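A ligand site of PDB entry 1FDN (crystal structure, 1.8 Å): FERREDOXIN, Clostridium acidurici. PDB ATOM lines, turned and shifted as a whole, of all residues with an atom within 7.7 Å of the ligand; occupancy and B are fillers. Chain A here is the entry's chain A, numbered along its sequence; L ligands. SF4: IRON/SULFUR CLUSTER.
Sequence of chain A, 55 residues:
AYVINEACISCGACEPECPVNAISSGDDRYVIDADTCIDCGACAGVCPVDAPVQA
An iron atom (FE3) of the ligand is bound by the side-chain sulfur (SG) of Cys 8 (2.2 Å). The side-chain sulfur (SG) of Cys 47 is bound to an iron atom (FE1) of the ligand (2.2 Å). The side-chain sulfur of Cys 14 is bound to an iron atom (FE2) of the ligand (2.2 Å). An iron atom (FE4) of the ligand is bound by the side-chain sulfur (SG) of Cys 11 (2.3 Å). N of Cys 14 sits close to S3 of the ligand (3.6 Å). A sulfur (S2) of the ligand sits close to the backbone NH (N) of Ile 9, 3.3 Å away. The backbone NH (N) of Gly 12 sits close to a sulfur (S1) of the ligand, at 3.2 Å. The backbone NH (N) of Cys 11 sits close to a sulfur (S1) of the ligand, at 3.5 Å.
The backbone carbonyl oxygen (O) of Asp 28 sits at hydrogen-bond distance from the side-chain hydroxyl (OG) of Ser 10 (3.5 Å). The side-chain sulfur of Cys 47 lies close to the backbone NH of Asp 50. SG of Cys 47 lies close to N of Val 49 (3.7 Å). SG of Cys 47 sits close to N of Ala 51, 3.3 Å away. The side-chain sulfur (SG) of Cys 8 lies close to the backbone NH (N) of Ser 10, at 3.3 Å. The backbone carbonyl oxygen (O) of Ile 4 lies within hydrogen-bond range of the guanidinium group (NH1) of Arg 29, 2.8 Å away. SG of Cys 8 lies close to N of Tyr 30 (3.6 Å). N of Ala 13 lies close to SG of Cys 11.
CG2 of Ile 4 touches S4 of the ligand, 3.8 Å away. Ser 10 touches the ligand (CA to S1, 3.9 Å). Tyr 30 touches the ligand. Val 49 touches the ligand. Pro 52 touches the ligand. 11 residues have an atom within 4 Å of the ligand: Ile 4, Cys 8, Ile 9, Ser 10, Cys 11, Gly 12, Cys 14, Tyr 30, Cys 47, Val 49 and Pro 52. Along chain A the residues within 4 Å of the ligand span positions 4 to 52.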
ATOM      1  N   VAL A   3     -19.212  27.294   9.259  1.00  0.00           N
ATOM      2  CA  VAL A   3     -19.879  26.011   9.199  1.00  0.00           C
ATOM      3  C   VAL A   3     -18.789  24.968   9.500  1.00  0.00           C
ATOM      4  O   VAL A   3     -17.622  25.134   9.130  1.00  0.00           O
ATOM      5  CB  VAL A   3     -20.516  25.837   7.774  1.00  0.00           C
ATOM      6  CG1 VAL A   3     -19.472  25.885   6.672  1.00  0.00           C
ATOM      7  CG2 VAL A   3     -21.253  24.512   7.720  1.00  0.00           C
ATOM      8  N   ILE A   4     -19.124  23.962  10.299  1.00  0.00           N
ATOM      9  CA  ILE A   4     -18.198  22.893  10.646  1.00  0.00           C
ATOM     10  C   ILE A   4     -18.251  21.890   9.518  1.00  0.00           C
ATOM     11  O   ILE A   4     -19.331  21.391   9.213  1.00  0.00           O
ATOM     12  CB  ILE A   4     -18.633  22.313  12.002  1.00  0.00           C
ATOM     13  CG1 ILE A   4     -18.353  23.376  13.058  1.00  0.00           C
ATOM     14  CG2 ILE A   4     -17.873  21.042  12.341  1.00  0.00           C
ATOM     15  CD1 ILE A   4     -18.843  23.079  14.477  1.00  0.00           C
ATOM     16  N   ASN A   5     -17.125  21.632   8.864  1.00  0.00           N
ATOM     17  CA  ASN A   5     -17.163  20.700   7.751  1.00  0.00           C
ATOM     18  C   ASN A   5     -16.920  19.253   8.180  1.00  0.00           C
ATOM     19  O   ASN A   5     -16.808  18.947   9.371  1.00  0.00           O
ATOM     20  CB  ASN A   5     -16.128  21.165   6.687  1.00  0.00           C
ATOM     21  CG  ASN A   5     -14.662  21.121   7.067  1.00  0.00           C
ATOM     22  OD1 ASN A   5     -14.232  20.336   7.908  1.00  0.00           O
ATOM     23  ND2 ASN A   5     -13.829  21.964   6.450  1.00  0.00           N
ATOM     24  N   ALA A   7     -14.372  17.283   8.348  1.00  0.00           N
ATOM     25  CA  ALA A   7     -13.179  16.910   9.081  1.00  0.00           C
ATOM     26  C   ALA A   7     -13.427  16.793  10.587  1.00  0.00           C
ATOM     27  O   ALA A   7     -12.590  16.193  11.261  1.00  0.00           O
ATOM     28  CB  ALA A   7     -12.087  17.947   8.837  1.00  0.00           C
ATOM     29  N   CYS A   8     -14.521  17.340  11.153  1.00  0.00           N
ATOM     30  CA  CYS A   8     -14.808  17.302  12.576  1.00  0.00           C
ATOM     31  C   CYS A   8     -14.733  15.893  13.146  1.00  0.00           C
ATOM     32  O   CYS A   8     -15.340  14.962  12.623  1.00  0.00           O
ATOM     33  CB  CYS A   8     -16.215  17.861  12.844  1.00  0.00           C
ATOM     34  SG  CYS A   8     -16.743  17.904  14.585  1.00  0.00           S
ATOM     35  N   ILE A   9     -13.971  15.768  14.240  1.00  0.00           N
ATOM     36  CA  ILE A   9     -13.857  14.493  14.909  1.00  0.00           C
ATOM     37  C   ILE A   9     -14.690  14.449  16.187  1.00  0.00           C
ATOM     38  O   ILE A   9     -14.499  13.561  17.018  1.00  0.00           O
ATOM     39  CB  ILE A   9     -12.349  14.172  15.223  1.00  0.00           C
ATOM     40  CG1 ILE A   9     -11.686  15.264  16.066  1.00  0.00           C
ATOM     41  CG2 ILE A   9     -11.629  13.956  13.893  1.00  0.00           C
ATOM     42  CD1 ILE A   9     -10.264  14.945  16.542  1.00  0.00           C
ATOM     43  N   SER A  10     -15.602  15.410  16.399  1.00  0.00           N
ATOM     44  CA  SER A  10     -16.488  15.452  17.567  1.00  0.00           C
ATOM     45  C   SER A  10     -15.819  15.392  18.935  1.00  0.00           C
ATOM     46  O   SER A  10     -16.286  14.769  19.900  1.00  0.00           O
ATOM     47  CB  SER A  10     -17.513  14.330  17.429  1.00  0.00           C
ATOM     48  OG  SER A  10     -18.340  14.555  16.299  1.00  0.00           O
ATOM     49  N   CYS A  11     -14.700  16.109  19.028  1.00  0.00           N
ATOM     50  CA  CYS A  11     -13.959  16.203  20.260  1.00  0.00           C
ATOM     51  C   CYS A  11     -14.638  17.091  21.306  1.00  0.00           C
ATOM     52  O   CYS A  11     -14.365  17.022  22.509  1.00  0.00           O
ATOM     53  CB  CYS A  11     -12.574  16.726  19.869  1.00  0.00           C
ATOM     54  SG  CYS A  11     -12.350  18.505  19.641  1.00  0.00           S
ATOM     55  N   GLY A  12     -15.493  18.024  20.859  1.00  0.00           N
ATOM     56  CA  GLY A  12     -16.225  18.876  21.766  1.00  0.00           C
ATOM     57  C   GLY A  12     -15.470  20.088  22.285  1.00  0.00           C
ATOM     58  O   GLY A  12     -16.055  20.903  23.005  1.00  0.00           O
ATOM     59  N   ALA A  13     -14.210  20.294  21.916  1.00  0.00           N
ATOM     60  CA  ALA A  13     -13.443  21.406  22.451  1.00  0.00           C
ATOM     61  C   ALA A  13     -13.930  22.822  22.095  1.00  0.00           C
ATOM     62  O   ALA A  13     -13.793  23.746  22.917  1.00  0.00           O
ATOM     63  CB  ALA A  13     -11.986  21.278  22.004  1.00  0.00           C
ATOM     64  N   CYS A  14     -14.593  22.967  20.931  1.00  0.00           N
ATOM     65  CA  CYS A  14     -15.053  24.254  20.498  1.00  0.00           C
ATOM     66  C   CYS A  14     -16.305  24.726  21.196  1.00  0.00           C
ATOM     67  O   CYS A  14     -16.455  25.931  21.414  1.00  0.00           O
ATOM     68  CB  CYS A  14     -15.361  24.281  19.012  1.00  0.00           C
ATOM     69  SG  CYS A  14     -16.486  22.955  18.525  1.00  0.00           S
ATOM     70  N   GLU A  15     -17.191  23.806  21.608  1.00  0.00           N
ATOM     71  CA  GLU A  15     -18.460  24.222  22.176  1.00  0.00           C
ATOM     72  C   GLU A  15     -18.399  25.211  23.336  1.00  0.00           C
ATOM     73  O   GLU A  15     -19.059  26.240  23.209  1.00  0.00           O
ATOM     74  CB  GLU A  15     -19.251  22.983  22.609  1.00  0.00           C
ATOM     75  CG  GLU A  15     -20.613  23.372  23.176  1.00  0.00           C
ATOM     76  CD  GLU A  15     -21.558  22.219  23.466  1.00  0.00           C
ATOM     77  OE1 GLU A  15     -21.113  21.180  23.953  1.00  0.00           O
ATOM     78  OE2 GLU A  15     -22.742  22.380  23.191  1.00  0.00           O
ATOM     79  N   ILE A  23     -22.613  26.827  19.097  1.00  0.00           N
ATOM     80  CA  ILE A  23     -22.245  25.464  18.746  1.00  0.00           C
ATOM     81  C   ILE A  23     -22.945  24.435  19.614  1.00  0.00           C
ATOM     82  O   ILE A  23     -23.043  24.613  20.831  1.00  0.00           O
ATOM     83  CB  ILE A  23     -20.696  25.298  18.886  1.00  0.00           C
ATOM     84  CG1 ILE A  23     -20.019  26.271  17.945  1.00  0.00           C
ATOM     85  CG2 ILE A  23     -20.250  23.849  18.586  1.00  0.00           C
ATOM     86  CD1 ILE A  23     -18.480  26.247  18.004  1.00  0.00           C
ATOM     87  N   SER A  24     -23.449  23.375  19.018  1.00  0.00           N
ATOM     88  CA  SER A  24     -23.970  22.252  19.761  1.00  0.00           C
ATOM     89  C   SER A  24     -23.526  20.937  19.114  1.00  0.00           C
ATOM     90  O   SER A  24     -23.002  20.894  17.987  1.00  0.00           O
ATOM     91  CB  SER A  24     -25.487  22.339  19.828  1.00  0.00           C
ATOM     92  OG  SER A  24     -26.109  22.321  18.550  1.00  0.00           O
ATOM     93  N   SER A  25     -23.658  19.849  19.860  1.00  0.00           N
ATOM     94  CA  SER A  25     -23.340  18.515  19.382  1.00  0.00           C
ATOM     95  C   SER A  25     -24.452  18.066  18.453  1.00  0.00           C
ATOM     96  O   SER A  25     -25.635  18.247  18.764  1.00  0.00           O
ATOM     97  CB  SER A  25     -23.225  17.601  20.588  1.00  0.00           C
ATOM     98  OG  SER A  25     -22.582  16.381  20.310  1.00  0.00           O
ATOM     99  N   ASP A  28     -23.180  12.999  13.774  1.00  0.00           N
ATOM    100  CA  ASP A  28     -22.023  12.974  12.876  1.00  0.00           C
ATOM    101  C   ASP A  28     -20.963  14.011  13.192  1.00  0.00           C
ATOM    102  O   ASP A  28     -19.792  13.639  13.279  1.00  0.00           O
ATOM    103  CB  ASP A  28     -22.392  13.157  11.403  1.00  0.00           C
ATOM    104  CG  ASP A  28     -22.848  11.899  10.646  1.00  0.00           C
ATOM    105  OD1 ASP A  28     -21.929  11.269  10.159  1.00  0.00           O
ATOM    106  OD2 ASP A  28     -24.028  11.585  10.571  1.00  0.00           O
ATOM    107  N   ARG A  29     -21.330  15.268  13.423  1.00  0.00           N
ATOM    108  CA  ARG A  29     -20.370  16.321  13.706  1.00  0.00           C
ATOM    109  C   ARG A  29     -21.101  17.379  14.510  1.00  0.00           C
ATOM    110  O   ARG A  29     -22.320  17.320  14.717  1.00  0.00           O
ATOM    111  CB  ARG A  29     -19.802  16.963  12.409  1.00  0.00           C
ATOM    112  CG  ARG A  29     -20.787  17.474  11.349  1.00  0.00           C
ATOM    113  CD  ARG A  29     -20.078  17.994  10.102  1.00  0.00           C
ATOM    114  NE  ARG A  29     -20.676  17.473   8.875  1.00  0.00           N
ATOM    115  CZ  ARG A  29     -20.981  18.221   7.798  1.00  0.00           C
ATOM    116  NH1 ARG A  29     -20.779  19.540   7.740  1.00  0.00           N
ATOM    117  NH2 ARG A  29     -21.503  17.643   6.729  1.00  0.00           N
ATOM    118  N   TYR A  30     -20.331  18.321  15.053  1.00  0.00           N
ATOM    119  CA  TYR A  30     -20.901  19.454  15.751  1.00  0.00           C
ATOM    120  C   TYR A  30     -21.527  20.433  14.750  1.00  0.00           C
ATOM    121  O   TYR A  30     -21.186  20.428  13.568  1.00  0.00           O
ATOM    122  CB  TYR A  30     -19.777  20.101  16.581  1.00  0.00           C
ATOM    123  CG  TYR A  30     -19.619  19.384  17.923  1.00  0.00           C
ATOM    124  CD1 TYR A  30     -19.252  18.034  17.990  1.00  0.00           C
ATOM    125  CD2 TYR A  30     -19.861  20.101  19.110  1.00  0.00           C
ATOM    126  CE1 TYR A  30     -19.130  17.395  19.232  1.00  0.00           C
ATOM    127  CE2 TYR A  30     -19.750  19.470  20.349  1.00  0.00           C
ATOM    128  CZ  TYR A  30     -19.386  18.120  20.392  1.00  0.00           C
ATOM    129  OH  TYR A  30     -19.334  17.497  21.616  1.00  0.00           O
ATOM    130  N   VAL A  31     -22.448  21.289  15.164  1.00  0.00           N
ATOM    131  CA  VAL A  31     -23.177  22.185  14.260  1.00  0.00           C
ATOM    132  C   VAL A  31     -23.168  23.613  14.753  1.00  0.00           C
ATOM    133  O   VAL A  31     -23.278  23.848  15.954  1.00  0.00           O
ATOM    134  CB  VAL A  31     -24.707  21.926  14.086  1.00  0.00           C
ATOM    135  CG1 VAL A  31     -24.947  21.789  12.606  1.00  0.00           C
ATOM    136  CG2 VAL A  31     -25.204  20.767  14.913  1.00  0.00           C
ATOM    137  N   ILE A  32     -23.071  24.546  13.814  1.00  0.00           N
ATOM    138  CA  ILE A  32     -23.158  25.961  14.126  1.00  0.00           C
ATOM    139  C   ILE A  32     -24.541  26.499  13.814  1.00  0.00           C
ATOM    140  O   ILE A  32     -25.126  26.226  12.762  1.00  0.00           O
ATOM    141  CB  ILE A  32     -22.080  26.715  13.317  1.00  0.00           C
ATOM    142  CG1 ILE A  32     -20.728  26.305  13.877  1.00  0.00           C
ATOM    143  CG2 ILE A  32     -22.283  28.246  13.377  1.00  0.00           C
ATOM    144  CD1 ILE A  32     -19.479  26.837  13.157  1.00  0.00           C
ATOM    145  N   CYS A  43     -13.791  29.179  17.315  1.00  0.00           N
ATOM    146  CA  CYS A  43     -13.939  27.732  17.197  1.00  0.00           C
ATOM    147  C   CYS A  43     -12.866  27.121  16.309  1.00  0.00           C
ATOM    148  O   CYS A  43     -12.287  26.094  16.647  1.00  0.00           O
ATOM    149  CB  CYS A  43     -15.310  27.379  16.629  1.00  0.00           C
ATOM    150  SG  CYS A  43     -15.812  28.356  15.200  1.00  0.00           S
ATOM    151  N   ALA A  44     -12.520  27.788  15.198  1.00  0.00           N
ATOM    152  CA  ALA A  44     -11.460  27.305  14.335  1.00  0.00           C
ATOM    153  C   ALA A  44     -10.116  27.333  15.077  1.00  0.00           C
ATOM    154  O   ALA A  44      -9.290  26.436  14.924  1.00  0.00           O
ATOM    155  CB  ALA A  44     -11.349  28.181  13.083  1.00  0.00           C
ATOM    156  N   GLY A  45      -9.898  28.326  15.950  1.00  0.00           N
ATOM    157  CA  GLY A  45      -8.666  28.455  16.709  1.00  0.00           C
ATOM    158  C   GLY A  45      -8.446  27.355  17.734  1.00  0.00           C
ATOM    159  O   GLY A  45      -7.313  27.083  18.127  1.00  0.00           O
ATOM    160  N   VAL A  46      -9.516  26.742  18.239  1.00  0.00           N
ATOM    161  CA  VAL A  46      -9.344  25.636  19.174  1.00  0.00           C
ATOM    162  C   VAL A  46      -9.630  24.276  18.535  1.00  0.00           C
ATOM    163  O   VAL A  46      -9.593  23.250  19.206  1.00  0.00           O
ATOM    164  CB  VAL A  46     -10.253  25.827  20.454  1.00  0.00           C
ATOM    165  CG1 VAL A  46      -9.758  27.063  21.203  1.00  0.00           C
ATOM    166  CG2 VAL A  46     -11.727  25.977  20.096  1.00  0.00           C
ATOM    167  N   CYS A  47      -9.827  24.237  17.215  1.00  0.00           N
ATOM    168  CA  CYS A  47     -10.081  23.004  16.525  1.00  0.00           C
ATOM    169  C   CYS A  47      -8.788  22.326  16.090  1.00  0.00           C
ATOM    170  O   CYS A  47      -8.083  22.839  15.224  1.00  0.00           O
ATOM    171  CB  CYS A  47     -10.921  23.237  15.302  1.00  0.00           C
ATOM    172  SG  CYS A  47     -11.464  21.654  14.601  1.00  0.00           S
ATOM    173  N   PRO A  48      -8.467  21.126  16.575  1.00  0.00           N
ATOM    174  CA  PRO A  48      -7.264  20.393  16.188  1.00  0.00           C
ATOM    175  C   PRO A  48      -7.190  20.081  14.691  1.00  0.00           C
ATOM    176  O   PRO A  48      -6.100  20.078  14.122  1.00  0.00           O
ATOM    177  CB  PRO A  48      -7.306  19.162  17.065  1.00  0.00           C
ATOM    178  CG  PRO A  48      -8.782  18.910  17.276  1.00  0.00           C
ATOM    179  CD  PRO A  48      -9.300  20.325  17.479  1.00  0.00           C
ATOM    180  N   VAL A  49      -8.338  19.830  14.068  1.00  0.00           N
ATOM    181  CA  VAL A  49      -8.391  19.464  12.663  1.00  0.00           C
ATOM    182  C   VAL A  49      -8.848  20.610  11.772  1.00  0.00           C
ATOM    183  O   VAL A  49      -9.084  20.402  10.586  1.00  0.00           O
ATOM    184  CB  VAL A  49      -9.334  18.234  12.482  1.00  0.00           C
ATOM    185  CG1 VAL A  49      -8.714  17.008  13.160  1.00  0.00           C
ATOM    186  CG2 VAL A  49     -10.719  18.510  13.067  1.00  0.00           C
ATOM    187  N   ASP A  50      -9.028  21.822  12.341  1.00  0.00           N
ATOM    188  CA  ASP A  50      -9.464  23.017  11.640  1.00  0.00           C
ATOM    189  C   ASP A  50     -10.742  22.840  10.815  1.00  0.00           C
ATOM    190  O   ASP A  50     -10.850  23.280   9.661  1.00  0.00           O
ATOM    191  CB  ASP A  50      -8.285  23.508  10.770  1.00  0.00           C
ATOM    192  CG  ASP A  50      -8.315  24.980  10.398  1.00  0.00           C
ATOM    193  OD1 ASP A  50      -8.611  25.833  11.241  1.00  0.00           O
ATOM    194  OD2 ASP A  50      -8.019  25.287   9.244  1.00  0.00           O
ATOM    195  N   ALA A  51     -11.743  22.183  11.405  1.00  0.00           N
ATOM    196  CA  ALA A  51     -13.001  21.956  10.705  1.00  0.00           C
ATOM    197  C   ALA A  51     -13.968  23.145  10.538  1.00  0.00           C
ATOM    198  O   ALA A  51     -14.691  23.136   9.526  1.00  0.00           O
ATOM    199  CB  ALA A  51     -13.762  20.829  11.414  1.00  0.00           C
ATOM    200  N   PRO A  52     -14.097  24.151  11.426  1.00  0.00           N
ATOM    201  CA  PRO A  52     -14.931  25.324  11.199  1.00  0.00           C
ATOM    202  C   PRO A  52     -14.326  26.192  10.096  1.00  0.00           C
ATOM    203  O   PRO A  52     -13.159  26.584  10.209  1.00  0.00           O
ATOM    204  CB  PRO A  52     -14.981  26.024  12.551  1.00  0.00           C
ATOM    205  CG  PRO A  52     -14.665  24.937  13.536  1.00  0.00           C
ATOM    206  CD  PRO A  52     -13.583  24.171  12.794  1.00  0.00           C
HETATM  207 FE1  SF4 L   1     -13.177  20.896  15.795  1.00  0.00          FE
HETATM  208 FE2  SF4 L   1     -15.320  21.431  17.378  1.00  0.00          FE
HETATM  209 FE3  SF4 L   1     -15.393  19.283  15.718  1.00  0.00          FE
HETATM  210 FE4  SF4 L   1     -13.643  19.269  17.930  1.00  0.00          FE
HETATM  211  S1  SF4 L   1     -15.883  19.268  17.947  1.00  0.00           S
HETATM  212  S2  SF4 L   1     -13.270  18.578  15.815  1.00  0.00           S
HETATM  213  S3  SF4 L   1     -13.151  21.446  18.005  1.00  0.00           S
HETATM  214  S4  SF4 L   1     -15.257  21.452  15.100  1.00  0.00           S
